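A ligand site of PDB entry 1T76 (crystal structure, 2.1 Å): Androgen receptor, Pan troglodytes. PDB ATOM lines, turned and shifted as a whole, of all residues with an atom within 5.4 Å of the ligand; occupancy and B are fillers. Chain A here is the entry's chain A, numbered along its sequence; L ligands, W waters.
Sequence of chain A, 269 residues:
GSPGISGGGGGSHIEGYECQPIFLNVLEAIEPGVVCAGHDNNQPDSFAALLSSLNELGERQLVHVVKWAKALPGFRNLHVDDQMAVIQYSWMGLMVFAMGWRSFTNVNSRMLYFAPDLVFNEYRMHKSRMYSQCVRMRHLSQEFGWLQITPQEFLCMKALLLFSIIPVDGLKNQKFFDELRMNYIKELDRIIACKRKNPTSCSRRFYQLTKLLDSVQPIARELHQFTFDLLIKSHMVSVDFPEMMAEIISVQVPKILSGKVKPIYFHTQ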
ATOM      1  N   LEU A  51       4.162 -24.963 -27.378  1.00  0.00           N
ATOM      2  CA  LEU A  51       4.088 -24.019 -26.266  1.00  0.00           C
ATOM      3  C   LEU A  51       5.382 -23.951 -25.470  1.00  0.00           C
ATOM      4  O   LEU A  51       5.755 -22.876 -24.998  1.00  0.00           O
ATOM      5  CB  LEU A  51       2.906 -24.365 -25.353  1.00  0.00           C
ATOM      6  CG  LEU A  51       1.564 -23.758 -25.810  1.00  0.00           C
ATOM      7  CD1 LEU A  51       1.615 -22.237 -25.649  1.00  0.00           C
ATOM      8  CD2 LEU A  51       1.283 -24.133 -27.268  1.00  0.00           C
ATOM      9  N   LEU A  54       7.567 -21.796 -27.461  1.00  0.00           N
ATOM     10  CA  LEU A  54       7.159 -20.389 -27.395  1.00  0.00           C
ATOM     11  C   LEU A  54       7.597 -19.803 -26.050  1.00  0.00           C
ATOM     12  O   LEU A  54       8.089 -18.677 -25.995  1.00  0.00           O
ATOM     13  CB  LEU A  54       5.649 -20.242 -27.567  1.00  0.00           C
ATOM     14  CG  LEU A  54       5.101 -20.315 -28.998  1.00  0.00           C
ATOM     15  CD1 LEU A  54       3.572 -20.358 -28.972  1.00  0.00           C
ATOM     16  CD2 LEU A  54       5.578 -19.093 -29.804  1.00  0.00           C
ATOM     17  N   ASN A  55       7.425 -20.557 -24.976  1.00  0.00           N
ATOM     18  CA  ASN A  55       7.827 -20.078 -23.655  1.00  0.00           C
ATOM     19  C   ASN A  55       9.338 -19.818 -23.626  1.00  0.00           C
ATOM     20  O   ASN A  55       9.774 -18.790 -23.104  1.00  0.00           O
ATOM     21  CB  ASN A  55       7.437 -21.072 -22.569  1.00  0.00           C
ATOM     22  CG  ASN A  55       5.959 -21.009 -22.222  1.00  0.00           C
ATOM     23  OD1 ASN A  55       5.331 -19.961 -22.345  1.00  0.00           O
ATOM     24  ND2 ASN A  55       5.397 -22.133 -21.773  1.00  0.00           N
ATOM     25  N   LEU A  57      11.218 -19.162 -26.153  1.00  0.00           N
ATOM     26  CA  LEU A  57      11.452 -17.994 -26.994  1.00  0.00           C
ATOM     27  C   LEU A  57      11.148 -16.723 -26.199  1.00  0.00           C
ATOM     28  O   LEU A  57      11.798 -15.689 -26.379  1.00  0.00           O
ATOM     29  CB  LEU A  57      10.562 -18.048 -28.239  1.00  0.00           C
ATOM     30  CG  LEU A  57      10.703 -16.821 -29.141  1.00  0.00           C
ATOM     31  CD1 LEU A  57      12.180 -16.648 -29.551  1.00  0.00           C
ATOM     32  CD2 LEU A  57       9.799 -16.976 -30.359  1.00  0.00           C
ATOM     33  N   GLY A  58      10.146 -16.791 -25.327  1.00  0.00           N
ATOM     34  CA  GLY A  58       9.814 -15.632 -24.520  1.00  0.00           C
ATOM     35  C   GLY A  58      10.937 -15.313 -23.553  1.00  0.00           C
ATOM     36  O   GLY A  58      11.269 -14.156 -23.331  1.00  0.00           O
ATOM     37  N   GLN A  61      13.793 -13.748 -25.660  1.00  0.00           N
ATOM     38  CA  GLN A  61      13.472 -12.398 -26.098  1.00  0.00           C
ATOM     39  C   GLN A  61      13.400 -11.438 -24.926  1.00  0.00           C
ATOM     40  O   GLN A  61      13.689 -10.251 -25.063  1.00  0.00           O
ATOM     41  CB  GLN A  61      12.160 -12.376 -26.876  1.00  0.00           C
ATOM     42  CG  GLN A  61      12.204 -13.189 -28.157  1.00  0.00           C
ATOM     43  CD  GLN A  61      11.154 -12.766 -29.159  1.00  0.00           C
ATOM     44  OE1 GLN A  61      10.989 -13.385 -30.198  1.00  0.00           O
ATOM     45  NE2 GLN A  61      10.438 -11.685 -28.843  1.00  0.00           N
ATOM     46  N   TRP A  91       6.092  -6.431 -21.811  1.00  0.00           N
ATOM     47  CA  TRP A  91       6.789  -7.378 -22.658  1.00  0.00           C
ATOM     48  C   TRP A  91       5.918  -8.085 -23.688  1.00  0.00           C
ATOM     49  O   TRP A  91       6.326  -8.265 -24.828  1.00  0.00           O
ATOM     50  CB  TRP A  91       7.565  -8.421 -21.838  1.00  0.00           C
ATOM     51  CG  TRP A  91       6.716  -9.315 -20.994  1.00  0.00           C
ATOM     52  CD1 TRP A  91       6.344  -9.094 -19.704  1.00  0.00           C
ATOM     53  CD2 TRP A  91       6.177 -10.583 -21.360  1.00  0.00           C
ATOM     54  NE1 TRP A  91       5.609 -10.154 -19.236  1.00  0.00           N
ATOM     55  CE2 TRP A  91       5.490 -11.084 -20.236  1.00  0.00           C
ATOM     56  CE3 TRP A  91       6.213 -11.354 -22.534  1.00  0.00           C
ATOM     57  CZ2 TRP A  91       4.846 -12.324 -20.249  1.00  0.00           C
ATOM     58  CZ3 TRP A  91       5.565 -12.580 -22.547  1.00  0.00           C
ATOM     59  CH2 TRP A  91       4.893 -13.062 -21.402  1.00  0.00           C
ATOM     60  N   MET A  92       4.722  -8.511 -23.287  1.00  0.00           N
ATOM     61  CA  MET A  92       3.820  -9.213 -24.211  1.00  0.00           C
ATOM     62  C   MET A  92       3.455  -8.368 -25.430  1.00  0.00           C
ATOM     63  O   MET A  92       3.527  -8.854 -26.560  1.00  0.00           O
ATOM     64  CB  MET A  92       2.538  -9.628 -23.502  1.00  0.00           C
ATOM     65  CG  MET A  92       1.606 -10.480 -24.369  1.00  0.00           C
ATOM     66  SD  MET A  92       2.238 -12.158 -24.649  1.00  0.00           S
ATOM     67  CE  MET A  92       1.816 -12.930 -23.075  1.00  0.00           C
ATOM     68  N   MET A  95       6.624  -7.773 -27.662  1.00  0.00           N
ATOM     69  CA  MET A  95       7.001  -8.954 -28.415  1.00  0.00           C
ATOM     70  C   MET A  95       6.028  -9.323 -29.510  1.00  0.00           C
ATOM     71  O   MET A  95       6.433  -9.807 -30.567  1.00  0.00           O
ATOM     72  CB  MET A  95       7.188 -10.137 -27.475  1.00  0.00           C
ATOM     73  CG  MET A  95       8.390  -9.986 -26.550  1.00  0.00           C
ATOM     74  SD  MET A  95       8.632 -11.441 -25.526  1.00  0.00           S
ATOM     75  CE  MET A  95       9.811 -10.763 -24.307  1.00  0.00           C
ATOM     76  N   VAL A  96       4.742  -9.103 -29.261  1.00  0.00           N
ATOM     77  CA  VAL A  96       3.724  -9.404 -30.261  1.00  0.00           C
ATOM     78  C   VAL A  96       3.857  -8.425 -31.412  1.00  0.00           C
ATOM     79  O   VAL A  96       3.783  -8.808 -32.586  1.00  0.00           O
ATOM     80  CB  VAL A  96       2.319  -9.281 -29.698  1.00  0.00           C
ATOM     81  CG1 VAL A  96       1.289  -9.319 -30.839  1.00  0.00           C
ATOM     82  CG2 VAL A  96       2.057 -10.397 -28.713  1.00  0.00           C
ATOM     83  N   MET A  99       6.899  -9.203 -33.459  1.00  0.00           N
ATOM     84  CA  MET A  99       6.652 -10.462 -34.147  1.00  0.00           C
ATOM     85  C   MET A  99       5.758 -10.176 -35.345  1.00  0.00           C
ATOM     86  O   MET A  99       5.941 -10.745 -36.418  1.00  0.00           O
ATOM     87  CB  MET A  99       5.957 -11.455 -33.215  1.00  0.00           C
ATOM     88  CG  MET A  99       5.744 -12.858 -33.782  1.00  0.00           C
ATOM     89  SD  MET A  99       4.351 -13.048 -34.937  1.00  0.00           S
ATOM     90  CE  MET A  99       2.944 -12.878 -33.820  1.00  0.00           C
ATOM     91  N   ARG A 102       7.915  -8.766 -38.052  1.00  0.00           N
ATOM     92  CA  ARG A 102       8.737  -9.799 -38.669  1.00  0.00           C
ATOM     93  C   ARG A 102       7.902 -10.591 -39.679  1.00  0.00           C
ATOM     94  O   ARG A 102       8.380 -10.912 -40.768  1.00  0.00           O
ATOM     95  CB  ARG A 102       9.263 -10.780 -37.633  1.00  0.00           C
ATOM     96  CG  ARG A 102      10.309 -10.240 -36.686  1.00  0.00           C
ATOM     97  CD  ARG A 102      11.038 -11.402 -36.017  1.00  0.00           C
ATOM     98  NE  ARG A 102      10.237 -12.110 -35.025  1.00  0.00           N
ATOM     99  CZ  ARG A 102       9.924 -11.604 -33.832  1.00  0.00           C
ATOM    100  NH1 ARG A 102      10.335 -10.392 -33.481  1.00  0.00           N
ATOM    101  NH2 ARG A 102       9.206 -12.331 -32.967  1.00  0.00           N
ATOM    102  N   PHE A 114       7.369 -16.141 -35.467  1.00  0.00           N
ATOM    103  CA  PHE A 114       7.837 -15.974 -34.092  1.00  0.00           C
ATOM    104  C   PHE A 114       9.371 -15.952 -34.048  1.00  0.00           C
ATOM    105  O   PHE A 114       9.969 -15.072 -33.428  1.00  0.00           O
ATOM    106  CB  PHE A 114       7.295 -17.120 -33.230  1.00  0.00           C
ATOM    107  CG  PHE A 114       5.804 -17.054 -32.979  1.00  0.00           C
ATOM    108  CD1 PHE A 114       5.271 -16.114 -32.109  1.00  0.00           C
ATOM    109  CD2 PHE A 114       4.938 -17.921 -33.647  1.00  0.00           C
ATOM    110  CE1 PHE A 114       3.895 -16.042 -31.878  1.00  0.00           C
ATOM    111  CE2 PHE A 114       3.557 -17.851 -33.429  1.00  0.00           C
ATOM    112  CZ  PHE A 114       3.029 -16.909 -32.546  1.00  0.00           C
ATOM    113  N   MET A 130      -4.418 -21.855 -29.507  1.00  0.00           N
ATOM    114  CA  MET A 130      -4.606 -20.417 -29.394  1.00  0.00           C
ATOM    115  C   MET A 130      -4.749 -19.858 -30.794  1.00  0.00           C
ATOM    116  O   MET A 130      -4.106 -18.872 -31.165  1.00  0.00           O
ATOM    117  CB  MET A 130      -3.449 -19.754 -28.637  1.00  0.00           C
ATOM    118  CG  MET A 130      -2.052 -20.139 -29.075  1.00  0.00           C
ATOM    119  SD  MET A 130      -0.786 -19.279 -28.082  1.00  0.00           S
ATOM    120  CE  MET A 130      -0.469 -17.833 -29.075  1.00  0.00           C
ATOM    121  N   MET A 137      -3.260 -11.782 -34.081  1.00  0.00           N
ATOM    122  CA  MET A 137      -1.869 -11.383 -34.283  1.00  0.00           C
ATOM    123  C   MET A 137      -1.578 -11.274 -35.770  1.00  0.00           C
ATOM    124  O   MET A 137      -0.883 -10.361 -36.200  1.00  0.00           O
ATOM    125  CB  MET A 137      -0.903 -12.382 -33.615  1.00  0.00           C
ATOM    126  CG  MET A 137      -0.950 -12.354 -32.083  1.00  0.00           C
ATOM    127  SD  MET A 137       0.345 -13.346 -31.302  1.00  0.00           S
ATOM    128  CE  MET A 137      -0.400 -14.958 -31.312  1.00  0.00           C
ATOM    129  N   LEU A 223      -3.573 -12.842 -24.746  1.00  0.00           N
ATOM    130  CA  LEU A 223      -2.407 -13.684 -24.568  1.00  0.00           C
ATOM    131  C   LEU A 223      -2.056 -13.783 -23.082  1.00  0.00           C
ATOM    132  O   LEU A 223      -1.602 -14.825 -22.621  1.00  0.00           O
ATOM    133  CB  LEU A 223      -1.229 -13.116 -25.370  1.00  0.00           C
ATOM    134  CG  LEU A 223      -1.435 -13.267 -26.885  1.00  0.00           C
ATOM    135  CD1 LEU A 223      -0.386 -12.510 -27.665  1.00  0.00           C
ATOM    136  CD2 LEU A 223      -1.402 -14.755 -27.235  1.00  0.00           C
ATOM    137  N   PHE A 226      -4.426 -16.220 -21.562  1.00  0.00           N
ATOM    138  CA  PHE A 226      -4.029 -17.542 -22.055  1.00  0.00           C
ATOM    139  C   PHE A 226      -2.772 -18.101 -21.381  1.00  0.00           C
ATOM    140  O   PHE A 226      -2.774 -19.249 -20.932  1.00  0.00           O
ATOM    141  CB  PHE A 226      -3.828 -17.492 -23.573  1.00  0.00           C
ATOM    142  CG  PHE A 226      -3.536 -18.847 -24.186  1.00  0.00           C
ATOM    143  CD1 PHE A 226      -2.242 -19.345 -24.213  1.00  0.00           C
ATOM    144  CD2 PHE A 226      -4.565 -19.617 -24.719  1.00  0.00           C
ATOM    145  CE1 PHE A 226      -1.969 -20.603 -24.754  1.00  0.00           C
ATOM    146  CE2 PHE A 226      -4.307 -20.879 -25.269  1.00  0.00           C
ATOM    147  CZ  PHE A 226      -2.998 -21.372 -25.287  1.00  0.00           C
ATOM    148  N   THR A 227      -1.713 -17.309 -21.300  1.00  0.00           N
ATOM    149  CA  THR A 227      -0.496 -17.828 -20.684  1.00  0.00           C
ATOM    150  C   THR A 227      -0.698 -18.050 -19.181  1.00  0.00           C
ATOM    151  O   THR A 227      -0.138 -18.999 -18.607  1.00  0.00           O
ATOM    152  CB  THR A 227       0.705 -16.881 -20.926  1.00  0.00           C
ATOM    153  OG1 THR A 227       1.907 -17.562 -20.569  1.00  0.00           O
ATOM    154  CG2 THR A 227       0.581 -15.605 -20.111  1.00  0.00           C
ATOM    155  N   LEU A 230      -2.447 -21.229 -18.728  1.00  0.00           N
ATOM    156  CA  LEU A 230      -1.508 -22.284 -19.067  1.00  0.00           C
ATOM    157  C   LEU A 230      -0.464 -22.523 -17.956  1.00  0.00           C
ATOM    158  O   LEU A 230      -0.075 -23.660 -17.718  1.00  0.00           O
ATOM    159  CB  LEU A 230      -0.790 -21.952 -20.382  1.00  0.00           C
ATOM    160  CG  LEU A 230       0.215 -22.987 -20.908  1.00  0.00           C
ATOM    161  CD1 LEU A 230      -0.389 -24.385 -20.892  1.00  0.00           C
ATOM    162  CD2 LEU A 230       0.630 -22.602 -22.316  1.00  0.00           C
ATOM    163  N   PHE A 241       7.687 -23.862 -18.407  1.00  0.00           N
ATOM    164  CA  PHE A 241       7.827 -22.410 -18.345  1.00  0.00           C
ATOM    165  C   PHE A 241       9.189 -22.069 -17.757  1.00  0.00           C
ATOM    166  O   PHE A 241       9.491 -22.452 -16.630  1.00  0.00           O
ATOM    167  CB  PHE A 241       6.752 -21.789 -17.443  1.00  0.00           C
ATOM    168  CG  PHE A 241       5.416 -21.603 -18.116  1.00  0.00           C
ATOM    169  CD1 PHE A 241       4.573 -22.676 -18.338  1.00  0.00           C
ATOM    170  CD2 PHE A 241       4.995 -20.321 -18.494  1.00  0.00           C
ATOM    171  CE1 PHE A 241       3.311 -22.489 -18.927  1.00  0.00           C
ATOM    172  CE2 PHE A 241       3.742 -20.131 -19.087  1.00  0.00           C
ATOM    173  CZ  PHE A 241       2.905 -21.210 -19.303  1.00  0.00           C
ATOM    174  N   MET A 245       9.817 -16.243 -16.972  1.00  0.00           N
ATOM    175  CA  MET A 245       8.451 -16.281 -17.469  1.00  0.00           C
ATOM    176  C   MET A 245       7.491 -16.690 -16.349  1.00  0.00           C
ATOM    177  O   MET A 245       6.492 -16.025 -16.100  1.00  0.00           O
ATOM    178  CB  MET A 245       8.348 -17.266 -18.639  1.00  0.00           C
ATOM    179  CG  MET A 245       9.035 -16.795 -19.929  1.00  0.00           C
ATOM    180  SD  MET A 245       8.045 -15.598 -20.879  1.00  0.00           S
ATOM    181  CE  MET A 245       8.782 -14.082 -20.393  1.00  0.00           C
ATOM    182  N   ILE A 249       4.674 -14.117 -14.970  1.00  0.00           N
ATOM    183  CA  ILE A 249       3.289 -14.486 -15.241  1.00  0.00           C
ATOM    184  C   ILE A 249       2.479 -14.766 -13.964  1.00  0.00           C
ATOM    185  O   ILE A 249       1.256 -14.654 -13.968  1.00  0.00           O
ATOM    186  CB  ILE A 249       3.240 -15.691 -16.202  1.00  0.00           C
ATOM    187  CG1 ILE A 249       3.844 -15.276 -17.557  1.00  0.00           C
ATOM    188  CG2 ILE A 249       1.802 -16.188 -16.378  1.00  0.00           C
ATOM    189  CD1 ILE A 249       4.232 -16.447 -18.448  1.00  0.00           C
HETATM  190  C1  LIG L   1       7.228 -15.070 -27.773  1.00  0.00           C
HETATM  191  C2  LIG L   1       7.965 -13.936 -28.501  1.00  0.00           C
HETATM  192  C3  LIG L   1       7.088 -13.534 -29.731  1.00  0.00           C
HETATM  193  O1  LIG L   1       7.633 -13.433 -30.814  1.00  0.00           O
HETATM  194  C4  LIG L   1       5.626 -13.303 -29.508  1.00  0.00           C
HETATM  195  C5  LIG L   1       4.950 -14.492 -28.784  1.00  0.00           C
HETATM  196  C6  LIG L   1       3.428 -14.235 -28.523  1.00  0.00           C
HETATM  197  C7  LIG L   1       2.808 -15.458 -27.825  1.00  0.00           C
HETATM  198  C8  LIG L   1       3.522 -15.800 -26.463  1.00  0.00           C
HETATM  199  C9  LIG L   1       5.047 -16.048 -26.734  1.00  0.00           C
HETATM  200  C10 LIG L   1       5.736 -14.803 -27.418  1.00  0.00           C
HETATM  201  C11 LIG L   1       5.724 -16.424 -25.374  1.00  0.00           C
HETATM  202  C12 LIG L   1       5.128 -17.594 -24.617  1.00  0.00           C
HETATM  203  C13 LIG L   1       3.593 -17.446 -24.429  1.00  0.00           C
HETATM  204  C14 LIG L   1       2.930 -17.051 -25.797  1.00  0.00           C
HETATM  205  C15 LIG L   1       1.435 -17.037 -25.421  1.00  0.00           C
HETATM  206  C16 LIG L   1       1.303 -18.329 -24.568  1.00  0.00           C
HETATM  207  C17 LIG L   1       2.761 -18.692 -24.164  1.00  0.00           C
HETATM  208  O2  LIG L   1       2.780 -19.097 -22.778  1.00  0.00           O
HETATM  209  C18 LIG L   1       3.338 -16.336 -23.322  1.00  0.00           C
HETATM  210  C19 LIG L   1       5.654 -13.566 -26.421  1.00  0.00           C
HETATM  211  O   HOH W   1       8.960 -10.400 -30.969  1.00  0.00           O
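O2 of the ligand is in hydrogen-bond range of OD1 of Asn 55, at 2.7 Å. O2 of the ligand lies within hydrogen-bond range of OG1 of Thr 227, at 2.8 Å. O1 of the ligand lies within hydrogen-bond range of NH2 of Arg 102, 2.9 Å away. OE1 of Gln 61 lies close to O1 of the ligand (3.4 Å).
ND2 of Asn 55 lies within hydrogen-bond range of O of Leu 51. OE1 of Gln 61 sits at hydrogen-bond distance from NH2 of Arg 102 (3.5 Å). NH2 of Arg 102 is in hydrogen-bond range of O of Phe 114, 2.9 Å away. The side-chain amide nitrogen of Gln 61 sits close to the side-chain sulfur of Met 95, at 3.8 Å.
Leu 54 touches the ligand (O to C11, 3.3 Å). Trp 91 touches the ligand. Met 92 touches the ligand (CE to C18, 3.7 Å). Met 95 touches the ligand. Met 99 touches the ligand (CB to O1, 3.5 Å). Phe 114 touches the ligand. Phe 226 touches the ligand (CD1 to C16, 3.7 Å). CE2 of Phe 241 touches O2 of the ligand (3.95 Å). Hydrophobic or aromatic side chains that line the ligand: Leu 54, Trp 91, Met 92, Met 95, Met 99, Phe 114, Phe 226 and Phe 241. Within 4 Å of the ligand: Leu 54, Asn 55, Gln 61, Trp 91, Met 92, Met 95, Met 99, Arg 102, Phe 114, Phe 226, Thr 227 and Phe 241. Along chain A the residues within 4 Å of the ligand span positions 54 to 241.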
